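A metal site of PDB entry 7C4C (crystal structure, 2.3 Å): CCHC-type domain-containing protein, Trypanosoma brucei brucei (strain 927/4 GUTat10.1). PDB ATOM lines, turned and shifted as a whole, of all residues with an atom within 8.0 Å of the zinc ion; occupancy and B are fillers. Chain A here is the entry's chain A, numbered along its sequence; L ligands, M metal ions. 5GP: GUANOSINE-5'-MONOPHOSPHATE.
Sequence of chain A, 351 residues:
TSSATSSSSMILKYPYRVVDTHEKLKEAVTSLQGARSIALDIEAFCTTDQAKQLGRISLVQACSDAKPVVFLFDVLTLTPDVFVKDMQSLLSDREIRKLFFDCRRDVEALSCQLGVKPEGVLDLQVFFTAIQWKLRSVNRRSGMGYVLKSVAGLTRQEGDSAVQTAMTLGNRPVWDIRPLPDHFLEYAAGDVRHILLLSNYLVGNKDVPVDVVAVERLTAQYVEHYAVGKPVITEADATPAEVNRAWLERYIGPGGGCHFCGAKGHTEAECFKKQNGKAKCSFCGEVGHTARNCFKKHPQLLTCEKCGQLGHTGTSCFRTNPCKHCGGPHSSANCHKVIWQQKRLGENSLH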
ATOM      1  N   GLY A 257       1.142  -8.402 -32.673  1.00  0.00           N
ATOM      2  CA  GLY A 257       1.757  -9.707 -32.580  1.00  0.00           C
ATOM      3  C   GLY A 257       1.607 -10.235 -31.179  1.00  0.00           C
ATOM      4  O   GLY A 257       0.835  -9.722 -30.370  1.00  0.00           O
ATOM      5  N   CYS A 258       2.413 -11.270 -30.888  1.00  0.00           N
ATOM      6  CA  CYS A 258       2.294 -12.029 -29.647  1.00  0.00           C
ATOM      7  C   CYS A 258       3.124 -11.379 -28.552  1.00  0.00           C
ATOM      8  O   CYS A 258       4.354 -11.391 -28.601  1.00  0.00           O
ATOM      9  CB  CYS A 258       2.734 -13.466 -29.858  1.00  0.00           C
ATOM     10  SG  CYS A 258       2.708 -14.380 -28.331  1.00  0.00           S
ATOM     11  N   HIS A 259       2.440 -10.846 -27.526  1.00  0.00           N
ATOM     12  CA  HIS A 259       3.127 -10.245 -26.393  1.00  0.00           C
ATOM     13  C   HIS A 259       3.895 -11.257 -25.553  1.00  0.00           C
ATOM     14  O   HIS A 259       4.703 -10.856 -24.721  1.00  0.00           O
ATOM     15  CB  HIS A 259       2.112  -9.516 -25.524  1.00  0.00           C
ATOM     16  CG  HIS A 259       1.521  -8.305 -26.162  1.00  0.00           C
ATOM     17  ND1 HIS A 259       0.565  -7.517 -25.549  1.00  0.00           N
ATOM     18  CD2 HIS A 259       1.756  -7.735 -27.366  1.00  0.00           C
ATOM     19  CE1 HIS A 259       0.242  -6.521 -26.354  1.00  0.00           C
ATOM     20  NE2 HIS A 259       0.957  -6.630 -27.464  1.00  0.00           N
ATOM     21  N   PHE A 260       3.665 -12.560 -25.743  1.00  0.00           N
ATOM     22  CA  PHE A 260       4.353 -13.558 -24.938  1.00  0.00           C
ATOM     23  C   PHE A 260       5.678 -13.982 -25.560  1.00  0.00           C
ATOM     24  O   PHE A 260       6.727 -13.907 -24.911  1.00  0.00           O
ATOM     25  CB  PHE A 260       3.463 -14.789 -24.732  1.00  0.00           C
ATOM     26  CG  PHE A 260       4.026 -15.765 -23.750  1.00  0.00           C
ATOM     27  CD1 PHE A 260       3.913 -15.541 -22.390  1.00  0.00           C
ATOM     28  CD2 PHE A 260       4.664 -16.906 -24.191  1.00  0.00           C
ATOM     29  CE1 PHE A 260       4.450 -16.445 -21.495  1.00  0.00           C
ATOM     30  CE2 PHE A 260       5.197 -17.818 -23.294  1.00  0.00           C
ATOM     31  CZ  PHE A 260       5.080 -17.594 -21.954  1.00  0.00           C
ATOM     32  N   CYS A 261       5.659 -14.433 -26.824  1.00  0.00           N
ATOM     33  CA  CYS A 261       6.869 -14.905 -27.495  1.00  0.00           C
ATOM     34  C   CYS A 261       7.520 -13.865 -28.400  1.00  0.00           C
ATOM     35  O   CYS A 261       8.717 -13.969 -28.658  1.00  0.00           O
ATOM     36  CB  CYS A 261       6.574 -16.177 -28.313  1.00  0.00           C
ATOM     37  SG  CYS A 261       5.564 -15.906 -29.763  1.00  0.00           S
ATOM     38  N   GLY A 262       6.791 -12.874 -28.880  1.00  0.00           N
ATOM     39  CA  GLY A 262       7.340 -11.847 -29.745  1.00  0.00           C
ATOM     40  C   GLY A 262       6.975 -11.955 -31.223  1.00  0.00           C
ATOM     41  O   GLY A 262       7.184 -10.994 -31.960  1.00  0.00           O
ATOM     42  N   ALA A 263       6.399 -13.076 -31.669  1.00  0.00           N
ATOM     43  CA  ALA A 263       6.230 -13.356 -33.095  1.00  0.00           C
ATOM     44  C   ALA A 263       4.960 -12.741 -33.655  1.00  0.00           C
ATOM     45  O   ALA A 263       3.907 -12.731 -33.009  1.00  0.00           O
ATOM     46  CB  ALA A 263       6.172 -14.861 -33.330  1.00  0.00           C
ATOM     47  N   LYS A 264       5.044 -12.268 -34.901  1.00  0.00           N
ATOM     48  CA  LYS A 264       3.834 -11.863 -35.587  1.00  0.00           C
ATOM     49  C   LYS A 264       3.054 -13.094 -36.024  1.00  0.00           C
ATOM     50  O   LYS A 264       3.570 -14.215 -36.043  1.00  0.00           O
ATOM     51  CB  LYS A 264       4.173 -10.984 -36.778  1.00  0.00           C
ATOM     52  CG  LYS A 264       5.262  -9.995 -36.455  1.00  0.00           C
ATOM     53  CD  LYS A 264       5.097  -8.701 -37.177  1.00  0.00           C
ATOM     54  CE  LYS A 264       6.031  -7.655 -36.578  1.00  0.00           C
ATOM     55  NZ  LYS A 264       5.760  -6.291 -37.105  1.00  0.00           N
ATOM     56  N   GLY A 265       1.771 -12.897 -36.319  1.00  0.00           N
ATOM     57  CA  GLY A 265       0.939 -13.953 -36.836  1.00  0.00           C
ATOM     58  C   GLY A 265      -0.006 -14.581 -35.839  1.00  0.00           C
ATOM     59  O   GLY A 265      -0.956 -15.266 -36.248  1.00  0.00           O
ATOM     60  N   HIS A 266       0.211 -14.381 -34.535  1.00  0.00           N
ATOM     61  CA  HIS A 266      -0.744 -14.883 -33.565  1.00  0.00           C
ATOM     62  C   HIS A 266      -0.732 -13.984 -32.347  1.00  0.00           C
ATOM     63  O   HIS A 266       0.187 -13.190 -32.145  1.00  0.00           O
ATOM     64  CB  HIS A 266      -0.461 -16.332 -33.164  1.00  0.00           C
ATOM     65  CG  HIS A 266       0.791 -16.514 -32.383  1.00  0.00           C
ATOM     66  ND1 HIS A 266       2.027 -16.723 -32.975  1.00  0.00           N
ATOM     67  CD2 HIS A 266       1.015 -16.516 -31.041  1.00  0.00           C
ATOM     68  CE1 HIS A 266       2.941 -16.846 -32.036  1.00  0.00           C
ATOM     69  NE2 HIS A 266       2.360 -16.731 -30.850  1.00  0.00           N
ATOM     70  N   THR A 267      -1.785 -14.104 -31.539  1.00  0.00           N
ATOM     71  CA  THR A 267      -1.921 -13.342 -30.303  1.00  0.00           C
ATOM     72  C   THR A 267      -1.521 -14.207 -29.115  1.00  0.00           C
ATOM     73  O   THR A 267      -1.380 -15.428 -29.204  1.00  0.00           O
ATOM     74  CB  THR A 267      -3.348 -12.839 -30.109  1.00  0.00           C
ATOM     75  OG1 THR A 267      -4.263 -13.943 -30.121  1.00  0.00           O
ATOM     76  CG2 THR A 267      -3.719 -11.868 -31.200  1.00  0.00           C
ATOM     77  N   GLU A 268      -1.361 -13.545 -27.969  1.00  0.00           N
ATOM     78  CA  GLU A 268      -0.963 -14.227 -26.748  1.00  0.00           C
ATOM     79  C   GLU A 268      -1.883 -15.400 -26.444  1.00  0.00           C
ATOM     80  O   GLU A 268      -1.429 -16.461 -26.012  1.00  0.00           O
ATOM     81  CB  GLU A 268      -0.942 -13.215 -25.603  1.00  0.00           C
ATOM     82  CG  GLU A 268      -0.555 -13.736 -24.277  1.00  0.00           C
ATOM     83  CD  GLU A 268      -0.143 -12.613 -23.350  1.00  0.00           C
ATOM     84  OE1 GLU A 268       0.633 -12.870 -22.415  1.00  0.00           O
ATOM     85  OE2 GLU A 268      -0.589 -11.460 -23.579  1.00  0.00           O
ATOM     86  N   ALA A 269      -3.184 -15.234 -26.685  1.00  0.00           N
ATOM     87  CA  ALA A 269      -4.149 -16.273 -26.380  1.00  0.00           C
ATOM     88  C   ALA A 269      -4.061 -17.466 -27.314  1.00  0.00           C
ATOM     89  O   ALA A 269      -4.644 -18.515 -27.014  1.00  0.00           O
ATOM     90  CB  ALA A 269      -5.570 -15.705 -26.432  1.00  0.00           C
ATOM     91  N   GLU A 270      -3.387 -17.332 -28.455  1.00  0.00           N
ATOM     92  CA  GLU A 270      -3.172 -18.440 -29.373  1.00  0.00           C
ATOM     93  C   GLU A 270      -1.777 -19.035 -29.266  1.00  0.00           C
ATOM     94  O   GLU A 270      -1.500 -20.038 -29.920  1.00  0.00           O
ATOM     95  CB  GLU A 270      -3.389 -17.982 -30.825  1.00  0.00           C
ATOM     96  CG  GLU A 270      -4.709 -17.261 -31.109  1.00  0.00           C
ATOM     97  CD  GLU A 270      -4.699 -16.536 -32.461  1.00  0.00           C
ATOM     98  OE1 GLU A 270      -3.745 -15.771 -32.745  1.00  0.00           O
ATOM     99  OE2 GLU A 270      -5.648 -16.740 -33.244  1.00  0.00           O
ATOM    100  N   CYS A 271      -0.896 -18.437 -28.467  1.00  0.00           N
ATOM    101  CA  CYS A 271       0.510 -18.812 -28.472  1.00  0.00           C
ATOM    102  C   CYS A 271       0.708 -20.230 -27.942  1.00  0.00           C
ATOM    103  O   CYS A 271       0.281 -20.544 -26.820  1.00  0.00           O
ATOM    104  CB  CYS A 271       1.318 -17.807 -27.655  1.00  0.00           C
ATOM    105  SG  CYS A 271       3.102 -18.157 -27.664  1.00  0.00           S
ATOM    106  N   PHE A 272       1.339 -21.109 -28.746  1.00  0.00           N
ATOM    107  CA  PHE A 272       1.660 -22.447 -28.270  1.00  0.00           C
ATOM    108  C   PHE A 272       2.740 -22.406 -27.209  1.00  0.00           C
ATOM    109  O   PHE A 272       2.676 -23.137 -26.223  1.00  0.00           O
ATOM    110  CB  PHE A 272       2.128 -23.376 -29.409  1.00  0.00           C
ATOM    111  CG  PHE A 272       1.307 -23.305 -30.664  1.00  0.00           C
ATOM    112  CD1 PHE A 272      -0.076 -23.208 -30.624  1.00  0.00           C
ATOM    113  CD2 PHE A 272       1.928 -23.389 -31.898  1.00  0.00           C
ATOM    114  CE1 PHE A 272      -0.812 -23.160 -31.793  1.00  0.00           C
ATOM    115  CE2 PHE A 272       1.196 -23.355 -33.068  1.00  0.00           C
ATOM    116  CZ  PHE A 272      -0.171 -23.231 -33.021  1.00  0.00           C
ATOM    117  N   LYS A 273       3.752 -21.561 -27.412  1.00  0.00           N
ATOM    118  CA  LYS A 273       4.819 -21.453 -26.419  1.00  0.00           C
ATOM    119  C   LYS A 273       4.269 -21.111 -25.033  1.00  0.00           C
ATOM    120  O   LYS A 273       4.842 -21.528 -24.018  1.00  0.00           O
ATOM    121  CB  LYS A 273       5.852 -20.427 -26.869  1.00  0.00           C
ATOM    122  CG  LYS A 273       6.731 -20.867 -28.015  1.00  0.00           C
ATOM    123  CD  LYS A 273       7.865 -19.870 -28.231  1.00  0.00           C
ATOM    124  CE  LYS A 273       8.543 -20.070 -29.569  1.00  0.00           C
ATOM    125  NZ  LYS A 273       9.779 -19.209 -29.725  1.00  0.00           N
ATOM    126  N   LYS A 274       3.170 -20.367 -24.963  1.00  0.00           N
ATOM    127  CA  LYS A 274       2.576 -20.077 -23.661  1.00  0.00           C
ATOM    128  C   LYS A 274       1.951 -21.326 -23.058  1.00  0.00           C
ATOM    129  O   LYS A 274       2.193 -21.644 -21.896  1.00  0.00           O
ATOM    130  CB  LYS A 274       1.561 -18.944 -23.768  1.00  0.00           C
ATOM    131  CG  LYS A 274       1.259 -18.271 -22.449  1.00  0.00           C
ATOM    132  CD  LYS A 274       0.513 -16.974 -22.607  1.00  0.00           C
ATOM    133  CE  LYS A 274      -0.089 -16.510 -21.282  1.00  0.00           C
ATOM    134  NZ  LYS A 274      -0.963 -15.309 -21.487  1.00  0.00           N
HETATM  135  C1' 5GP L   1       1.283 -20.346 -37.495  1.00  0.00           C
HETATM  136  N9  5GP L   1       1.753 -20.251 -36.089  1.00  0.00           N
HETATM  137  C8  5GP L   1       3.029 -20.203 -35.719  1.00  0.00           C
HETATM  138  N7  5GP L   1       3.156 -20.101 -34.387  1.00  0.00           N
HETATM  139  C5  5GP L   1       1.925 -20.115 -33.879  1.00  0.00           C
HETATM  140  C6  5GP L   1       1.335 -20.036 -32.529  1.00  0.00           C
HETATM  141  O6  5GP L   1       2.040 -19.971 -31.526  1.00  0.00           O
HETATM  142  N1  5GP L   1       0.038 -20.043 -32.426  1.00  0.00           N
HETATM  143  C2  5GP L   1      -0.759 -20.134 -33.482  1.00  0.00           C
HETATM  144  N2  5GP L   1      -2.079 -20.164 -33.262  1.00  0.00           N
HETATM  145  N3  5GP L   1      -0.313 -20.213 -34.753  1.00  0.00           N
HETATM  146  C4  5GP L   1       1.010 -20.210 -35.004  1.00  0.00           C
HETATM  147 ZN    ZN M   1       3.493 -16.409 -29.114  1.00  0.00          ZN
HETATM  148 MN    MN M   2       5.583 -20.268 -32.921  1.00  0.00          MN
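SG of Cys 271 lies close to N of Lys 274 (3.5 Å).
N of Cys 258 is in hydrogen-bond range of O of Ala 263.
The side-chain sulfur of Cys 271 lies close to the backbone NH of Lys 273.
The backbone NH (N) of Phe 260 sits close to the side-chain sulfur (SG) of Cys 258 (3.3 Å).
The backbone NH (N) of Ala 263 lies close to the side-chain sulfur (SG) of Cys 261 (3.5 Å).
Of the 18 residues printed, 4 come within 4 Å of the zinc ion.
The nearest printed residue that does not touch the zinc ion is Phe 260 (4.7 Å).
A ring nitrogen (NE2) of His 266 binds the zinc ion (2.1 Å).
The side-chain sulfur (SG) of Cys 261 is bound to the zinc ion (2.2 Å).
The side-chain sulfur (SG) of Cys 271 is bound to the zinc ion (2.3 Å).
The zinc ion is bound by the side-chain sulfur (SG) of Cys 258, at 2.3 Å.
A ring nitrogen (NE2) of His 266 sits close to an oxygen (O6) of the ligand, 3.3 Å away.
An oxygen (O6) of the ligand sits at hydrogen-bond distance from the backbone NH of Phe 272 (3.1 Å).
The backbone carbonyl oxygen of Glu 270 lies within hydrogen-bond range of a nitrogen (N1) of the ligand.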
